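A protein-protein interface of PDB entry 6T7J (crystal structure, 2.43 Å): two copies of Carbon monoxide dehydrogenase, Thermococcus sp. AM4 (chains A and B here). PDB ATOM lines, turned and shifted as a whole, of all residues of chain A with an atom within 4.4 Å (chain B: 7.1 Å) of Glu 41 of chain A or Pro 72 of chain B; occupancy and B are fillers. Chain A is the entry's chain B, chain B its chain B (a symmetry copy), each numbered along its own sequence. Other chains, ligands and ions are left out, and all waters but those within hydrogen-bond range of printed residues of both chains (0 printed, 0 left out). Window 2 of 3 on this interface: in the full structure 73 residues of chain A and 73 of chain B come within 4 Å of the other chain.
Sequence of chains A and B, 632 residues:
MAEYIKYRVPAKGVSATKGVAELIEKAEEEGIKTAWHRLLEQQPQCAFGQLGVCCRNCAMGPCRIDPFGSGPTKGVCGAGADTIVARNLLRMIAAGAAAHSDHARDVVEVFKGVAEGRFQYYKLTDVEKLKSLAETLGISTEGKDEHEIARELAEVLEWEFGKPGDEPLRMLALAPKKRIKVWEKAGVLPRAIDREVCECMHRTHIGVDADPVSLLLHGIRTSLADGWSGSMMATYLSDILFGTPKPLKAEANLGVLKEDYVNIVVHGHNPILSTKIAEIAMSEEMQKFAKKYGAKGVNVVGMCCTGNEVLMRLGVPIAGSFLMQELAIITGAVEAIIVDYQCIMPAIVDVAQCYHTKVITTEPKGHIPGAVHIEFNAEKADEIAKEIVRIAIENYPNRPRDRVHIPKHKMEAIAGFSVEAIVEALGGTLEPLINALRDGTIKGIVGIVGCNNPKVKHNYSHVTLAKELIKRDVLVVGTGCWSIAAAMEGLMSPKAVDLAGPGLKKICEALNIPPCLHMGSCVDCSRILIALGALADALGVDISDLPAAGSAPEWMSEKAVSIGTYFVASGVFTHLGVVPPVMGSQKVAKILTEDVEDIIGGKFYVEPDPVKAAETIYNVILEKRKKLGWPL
The guanidinium group (NE) of Arg 38 of chain A sits at hydrogen-bond distance from the backbone carbonyl oxygen (O) of Gly 75 of chain B (3.1 Å). N of Arg 64 of chain B lies within hydrogen-bond range of OE1 of Gln 42 of chain A (3.0 Å). The side-chain amide nitrogen (NE2) of Gln 42 of chain A is in hydrogen-bond range of the backbone carbonyl oxygen (O) of Lys 74 of chain B (3.4 Å).
The backbone carbonyl oxygen (O) of Lys 33 of chain A is in hydrogen-bond range of the guanidinium group (NH1) of Arg 38 of chain A, 3.1 Å away. NZ of Lys 33 of chain A is in salt-bridge range of OE2 of Glu 41 of chain A, at 2.5 Å. The backbone NH (N) of Asp 66 of chain B is in hydrogen-bond range of the backbone carbonyl oxygen (O) of Pro 72 of chain B (2.9 Å).
Among the printed residues, merely in contact across the chains: Glu 41 of chain A with Pro 72 of chain B, Gln 42 of chain A with Cys 63 of chain B, Gln 42 of chain A with Pro 72 of chain B and Gln 42 of chain A with Gly 75 of chain B.
Glu 41 of chain A touches just one residue of chain B: Pro 72. Printed residues of chain B within 4 Å of Gln 42 of chain A: Cys 63 (3.3 Å), Arg 64 (3.0 Å), Pro 72 (3.8 Å), Lys 74 (3.4 Å) and Gly 75 (3.9 Å). Of the printed residues of chain A, Arg 64 of chain B touches Gln 42 (3.0 Å). Ile 65 of chain B touches none of the printed residues of chain A. Gly 69 of chain B touches none of the printed residues of chain A. Pro 72 of chain B touches just these residues of chain A: Glu 41 and Gln 42. Of the printed residues of chain A, Lys 74 of chain B touches Gln 42. Of the printed residues of chain A, Gly 75 of chain B touches Arg 38 and Gln 42. The nearest printed residue of chain A that does not touch Pro 72 of chain B is Arg 38 of chain A (5.8 Å).
Of the 13 printed residues of chain B, 5 touch a printed residue of chain A. Of the 9 printed residues of chain A, 3 touch a printed residue of chain B. Printed residues of chain A that touch a printed residue of chain B: Arg 38, Glu 41 and Gln 42.
No position is printed for both chains.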
ATOM      1  N   TYR A   7      10.530   5.235  -0.818  1.00  0.00           N
ATOM      2  CA  TYR A   7       9.556   6.246  -1.213  1.00  0.00           C
ATOM      3  C   TYR A   7       9.930   7.574  -0.576  1.00  0.00           C
ATOM      4  O   TYR A   7      10.144   7.646   0.639  1.00  0.00           O
ATOM      5  CB  TYR A   7       8.128   5.852  -0.807  1.00  0.00           C
ATOM      6  CG  TYR A   7       7.759   4.427  -1.144  1.00  0.00           C
ATOM      7  CD1 TYR A   7       7.012   4.127  -2.276  1.00  0.00           C
ATOM      8  CD2 TYR A   7       8.152   3.379  -0.325  1.00  0.00           C
ATOM      9  CE1 TYR A   7       6.675   2.822  -2.583  1.00  0.00           C
ATOM     10  CE2 TYR A   7       7.815   2.076  -0.620  1.00  0.00           C
ATOM     11  CZ  TYR A   7       7.085   1.801  -1.751  1.00  0.00           C
ATOM     12  OH  TYR A   7       6.759   0.497  -2.042  1.00  0.00           O
ATOM     13  N   LYS A  33      16.062   7.389   7.186  1.00  0.00           N
ATOM     14  CA  LYS A  33      14.611   7.258   7.201  1.00  0.00           C
ATOM     15  C   LYS A  33      14.024   7.971   8.411  1.00  0.00           C
ATOM     16  O   LYS A  33      14.531   7.840   9.529  1.00  0.00           O
ATOM     17  CB  LYS A  33      14.205   5.784   7.218  1.00  0.00           C
ATOM     18  CG  LYS A  33      14.706   4.974   6.033  1.00  0.00           C
ATOM     19  CD  LYS A  33      13.961   3.650   5.923  1.00  0.00           C
ATOM     20  CE  LYS A  33      14.677   2.683   4.996  1.00  0.00           C
ATOM     21  NZ  LYS A  33      13.862   1.471   4.717  1.00  0.00           N
ATOM     22  N   HIS A  37       8.845   8.360   6.069  1.00  0.00           N
ATOM     23  CA  HIS A  37       9.276   7.341   5.116  1.00  0.00           C
ATOM     24  C   HIS A  37       8.786   5.958   5.526  1.00  0.00           C
ATOM     25  O   HIS A  37       8.323   5.177   4.686  1.00  0.00           O
ATOM     26  CB  HIS A  37      10.800   7.348   4.989  1.00  0.00           C
ATOM     27  CG  HIS A  37      11.371   8.678   4.608  1.00  0.00           C
ATOM     28  ND1 HIS A  37      11.849   9.578   5.536  1.00  0.00           N
ATOM     29  CD2 HIS A  37      11.543   9.261   3.397  1.00  0.00           C
ATOM     30  CE1 HIS A  37      12.288  10.658   4.915  1.00  0.00           C
ATOM     31  NE2 HIS A  37      12.112  10.491   3.616  1.00  0.00           N
ATOM     32  N   ARG A  38       8.870   5.637   6.818  1.00  0.00           N
ATOM     33  CA  ARG A  38       8.437   4.322   7.271  1.00  0.00           C
ATOM     34  C   ARG A  38       6.919   4.191   7.241  1.00  0.00           C
ATOM     35  O   ARG A  38       6.397   3.104   6.959  1.00  0.00           O
ATOM     36  CB  ARG A  38       8.996   4.047   8.666  1.00  0.00           C
ATOM     37  CG  ARG A  38      10.523   3.988   8.691  1.00  0.00           C
ATOM     38  CD  ARG A  38      11.058   3.550  10.041  1.00  0.00           C
ATOM     39  NE  ARG A  38      10.738   4.517  11.086  1.00  0.00           N
ATOM     40  CZ  ARG A  38      11.523   5.534  11.431  1.00  0.00           C
ATOM     41  NH1 ARG A  38      12.683   5.718  10.815  1.00  0.00           N
ATOM     42  NH2 ARG A  38      11.144   6.367  12.390  1.00  0.00           N
ATOM     43  N   LEU A  39       6.194   5.283   7.508  1.00  0.00           N
ATOM     44  CA  LEU A  39       4.752   5.280   7.283  1.00  0.00           C
ATOM     45  C   LEU A  39       4.428   4.952   5.832  1.00  0.00           C
ATOM     46  O   LEU A  39       3.529   4.149   5.553  1.00  0.00           O
ATOM     47  CB  LEU A  39       4.148   6.630   7.666  1.00  0.00           C
ATOM     48  CG  LEU A  39       2.692   6.818   7.229  1.00  0.00           C
ATOM     49  CD1 LEU A  39       1.780   5.874   8.001  1.00  0.00           C
ATOM     50  CD2 LEU A  39       2.245   8.266   7.400  1.00  0.00           C
ATOM     51  N   LEU A  40       5.151   5.570   4.892  1.00  0.00           N
ATOM     52  CA  LEU A  40       4.959   5.246   3.481  1.00  0.00           C
ATOM     53  C   LEU A  40       5.274   3.781   3.205  1.00  0.00           C
ATOM     54  O   LEU A  40       4.595   3.129   2.403  1.00  0.00           O
ATOM     55  CB  LEU A  40       5.829   6.154   2.608  1.00  0.00           C
ATOM     56  CG  LEU A  40       5.415   7.624   2.519  1.00  0.00           C
ATOM     57  CD1 LEU A  40       6.352   8.391   1.596  1.00  0.00           C
ATOM     58  CD2 LEU A  40       3.974   7.746   2.052  1.00  0.00           C
ATOM     59  N   GLU A  41       6.306   3.247   3.861  1.00  0.00           N
ATOM     60  CA  GLU A  41       6.645   1.838   3.685  1.00  0.00           C
ATOM     61  C   GLU A  41       5.559   0.919   4.234  1.00  0.00           C
ATOM     62  O   GLU A  41       5.425  -0.222   3.777  1.00  0.00           O
ATOM     63  CB  GLU A  41       7.984   1.529   4.356  1.00  0.00           C
ATOM     64  CG  GLU A  41       9.184   2.156   3.670  1.00  0.00           C
ATOM     65  CD  GLU A  41      10.471   1.413   3.960  1.00  0.00           C
ATOM     66  OE1 GLU A  41      10.399   0.236   4.371  1.00  0.00           O
ATOM     67  OE2 GLU A  41      11.556   2.004   3.779  1.00  0.00           O
ATOM     68  N   GLN A  42       4.784   1.387   5.213  1.00  0.00           N
ATOM     69  CA  GLN A  42       3.727   0.561   5.788  1.00  0.00           C
ATOM     70  C   GLN A  42       2.472   0.510   4.925  1.00  0.00           C
ATOM     71  O   GLN A  42       1.634  -0.374   5.133  1.00  0.00           O
ATOM     72  CB  GLN A  42       3.354   1.071   7.184  1.00  0.00           C
ATOM     73  CG  GLN A  42       4.400   0.792   8.251  1.00  0.00           C
ATOM     74  CD  GLN A  42       4.608  -0.692   8.495  1.00  0.00           C
ATOM     75  OE1 GLN A  42       3.688  -1.496   8.335  1.00  0.00           O
ATOM     76  NE2 GLN A  42       5.822  -1.061   8.885  1.00  0.00           N
ATOM     77  N   GLN A  43       2.327   1.420   3.964  1.00  0.00           N
ATOM     78  CA  GLN A  43       1.038   1.507   3.286  1.00  0.00           C
ATOM     79  C   GLN A  43       0.993   0.579   2.073  1.00  0.00           C
ATOM     80  O   GLN A  43       1.997   0.424   1.371  1.00  0.00           O
ATOM     81  CB  GLN A  43       0.760   2.941   2.845  1.00  0.00           C
ATOM     82  CG  GLN A  43       0.209   3.818   3.955  1.00  0.00           C
ATOM     83  CD  GLN A  43       0.600   5.271   3.798  1.00  0.00           C
ATOM     84  OE1 GLN A  43       1.504   5.601   3.030  1.00  0.00           O
ATOM     85  NE2 GLN A  43      -0.080   6.151   4.527  1.00  0.00           N
ATOM     86  N   PHE B  48       1.495 -12.500   9.787  1.00  0.00           N
ATOM     87  CA  PHE B  48       2.172 -11.482  10.585  1.00  0.00           C
ATOM     88  C   PHE B  48       1.744 -11.556  12.044  1.00  0.00           C
ATOM     89  O   PHE B  48       2.583 -11.529  12.951  1.00  0.00           O
ATOM     90  CB  PHE B  48       1.895 -10.095  10.005  1.00  0.00           C
ATOM     91  CG  PHE B  48       2.271  -9.959   8.557  1.00  0.00           C
ATOM     92  CD1 PHE B  48       3.573  -9.657   8.191  1.00  0.00           C
ATOM     93  CD2 PHE B  48       1.324 -10.142   7.562  1.00  0.00           C
ATOM     94  CE1 PHE B  48       3.924  -9.535   6.861  1.00  0.00           C
ATOM     95  CE2 PHE B  48       1.668 -10.024   6.229  1.00  0.00           C
ATOM     96  CZ  PHE B  48       2.970  -9.719   5.878  1.00  0.00           C
ATOM     97  N   CYS B  63       1.380  -1.714  12.117  1.00  0.00           N
ATOM     98  CA  CYS B  63       2.642  -1.902  11.417  1.00  0.00           C
ATOM     99  C   CYS B  63       2.982  -3.383  11.345  1.00  0.00           C
ATOM    100  O   CYS B  63       2.860  -4.110  12.338  1.00  0.00           O
ATOM    101  CB  CYS B  63       3.798  -1.161  12.103  1.00  0.00           C
ATOM    102  SG  CYS B  63       3.931   0.615  11.867  1.00  0.00           S
ATOM    103  N   ARG B  64       3.427  -3.807  10.165  1.00  0.00           N
ATOM    104  CA  ARG B  64       3.890  -5.160   9.893  1.00  0.00           C
ATOM    105  C   ARG B  64       5.397  -5.153   9.699  1.00  0.00           C
ATOM    106  O   ARG B  64       5.938  -4.264   9.034  1.00  0.00           O
ATOM    107  CB  ARG B  64       3.261  -5.719   8.617  1.00  0.00           C
ATOM    108  CG  ARG B  64       1.814  -6.114   8.687  1.00  0.00           C
ATOM    109  CD  ARG B  64       1.214  -5.905   7.312  1.00  0.00           C
ATOM    110  NE  ARG B  64       0.001  -6.680   7.086  1.00  0.00           N
ATOM    111  CZ  ARG B  64      -0.757  -6.557   6.001  1.00  0.00           C
ATOM    112  NH1 ARG B  64      -0.422  -5.693   5.052  1.00  0.00           N
ATOM    113  NH2 ARG B  64      -1.849  -7.298   5.866  1.00  0.00           N
ATOM    114  N   ILE B  65       6.072  -6.160  10.239  1.00  0.00           N
ATOM    115  CA  ILE B  65       7.483  -6.385   9.953  1.00  0.00           C
ATOM    116  C   ILE B  65       7.582  -7.642   9.107  1.00  0.00           C
ATOM    117  O   ILE B  65       7.102  -8.709   9.508  1.00  0.00           O
ATOM    118  CB  ILE B  65       8.322  -6.509  11.233  1.00  0.00           C
ATOM    119  CG1 ILE B  65       8.154  -5.262  12.101  1.00  0.00           C
ATOM    120  CG2 ILE B  65       9.787  -6.714  10.878  1.00  0.00           C
ATOM    121  CD1 ILE B  65       8.248  -3.961  11.334  1.00  0.00           C
ATOM    122  N   ASP B  66       8.194  -7.517   7.931  1.00  0.00           N
ATOM    123  CA  ASP B  66       8.335  -8.650   7.030  1.00  0.00           C
ATOM    124  C   ASP B  66       9.569  -9.457   7.413  1.00  0.00           C
ATOM    125  O   ASP B  66      10.698  -8.992   7.173  1.00  0.00           O
ATOM    126  CB  ASP B  66       8.422  -8.182   5.586  1.00  0.00           C
ATOM    127  CG  ASP B  66       8.618  -9.328   4.616  1.00  0.00           C
ATOM    128  OD1 ASP B  66       7.650 -10.078   4.366  1.00  0.00           O
ATOM    129  OD2 ASP B  66       9.746  -9.480   4.109  1.00  0.00           O
ATOM    130  N   PRO B  67       9.420 -10.648   7.996  1.00  0.00           N
ATOM    131  CA  PRO B  67      10.598 -11.455   8.342  1.00  0.00           C
ATOM    132  C   PRO B  67      11.290 -12.048   7.129  1.00  0.00           C
ATOM    133  O   PRO B  67      12.465 -12.424   7.228  1.00  0.00           O
ATOM    134  CB  PRO B  67      10.021 -12.546   9.251  1.00  0.00           C
ATOM    135  CG  PRO B  67       8.613 -12.708   8.774  1.00  0.00           C
ATOM    136  CD  PRO B  67       8.157 -11.359   8.274  1.00  0.00           C
ATOM    137  N   GLY B  69      12.164 -10.245   4.739  1.00  0.00           N
ATOM    138  CA  GLY B  69      13.000  -9.185   4.227  1.00  0.00           C
ATOM    139  C   GLY B  69      12.470  -8.550   2.962  1.00  0.00           C
ATOM    140  O   GLY B  69      13.104  -7.625   2.438  1.00  0.00           O
ATOM    141  N   SER B  70      11.326  -9.025   2.460  1.00  0.00           N
ATOM    142  CA  SER B  70      10.722  -8.466   1.254  1.00  0.00           C
ATOM    143  C   SER B  70      10.403  -6.989   1.434  1.00  0.00           C
ATOM    144  O   SER B  70      10.897  -6.134   0.687  1.00  0.00           O
ATOM    145  CB  SER B  70       9.449  -9.242   0.905  1.00  0.00           C
ATOM    146  OG  SER B  70       9.588 -10.622   1.189  1.00  0.00           O
ATOM    147  N   GLY B  71       9.570  -6.673   2.419  1.00  0.00           N
ATOM    148  CA  GLY B  71       9.094  -5.327   2.617  1.00  0.00           C
ATOM    149  C   GLY B  71       9.684  -4.657   3.839  1.00  0.00           C
ATOM    150  O   GLY B  71      10.887  -4.744   4.110  1.00  0.00           O
ATOM    151  N   PRO B  72       8.834  -3.980   4.611  1.00  0.00           N
ATOM    152  CA  PRO B  72       9.337  -3.129   5.696  1.00  0.00           C
ATOM    153  C   PRO B  72       9.957  -3.942   6.820  1.00  0.00           C
ATOM    154  O   PRO B  72       9.431  -4.980   7.228  1.00  0.00           O
ATOM    155  CB  PRO B  72       8.083  -2.387   6.173  1.00  0.00           C
ATOM    156  CG  PRO B  72       6.959  -3.301   5.827  1.00  0.00           C
ATOM    157  CD  PRO B  72       7.362  -4.001   4.555  1.00  0.00           C
ATOM    158  N   THR B  73      11.089  -3.451   7.321  1.00  0.00           N
ATOM    159  CA  THR B  73      11.784  -4.077   8.436  1.00  0.00           C
ATOM    160  C   THR B  73      11.568  -3.352   9.758  1.00  0.00           C
ATOM    161  O   THR B  73      11.945  -3.887  10.806  1.00  0.00           O
ATOM    162  CB  THR B  73      13.290  -4.160   8.147  1.00  0.00           C
ATOM    163  OG1 THR B  73      13.908  -2.903   8.451  1.00  0.00           O
ATOM    164  CG2 THR B  73      13.534  -4.497   6.685  1.00  0.00           C
ATOM    165  N   LYS B  74      10.974  -2.161   9.740  1.00  0.00           N
ATOM    166  CA  LYS B  74      10.764  -1.385  10.953  1.00  0.00           C
ATOM    167  C   LYS B  74       9.413  -0.688  10.888  1.00  0.00           C
ATOM    168  O   LYS B  74       8.959  -0.277   9.817  1.00  0.00           O
ATOM    169  CB  LYS B  74      11.883  -0.358  11.158  1.00  0.00           C
ATOM    170  CG  LYS B  74      13.182  -0.969  11.648  1.00  0.00           C
ATOM    171  CD  LYS B  74      14.301   0.039  11.658  1.00  0.00           C
ATOM    172  CE  LYS B  74      15.158  -0.171  12.873  1.00  0.00           C
ATOM    173  NZ  LYS B  74      15.637   1.117  13.305  1.00  0.00           N
ATOM    174  N   GLY B  75       8.772  -0.562  12.047  1.00  0.00           N
ATOM    175  CA  GLY B  75       7.511   0.141  12.142  1.00  0.00           C
ATOM    176  C   GLY B  75       7.689   1.644  12.006  1.00  0.00           C
ATOM    177  O   GLY B  75       8.797   2.170  11.883  1.00  0.00           O
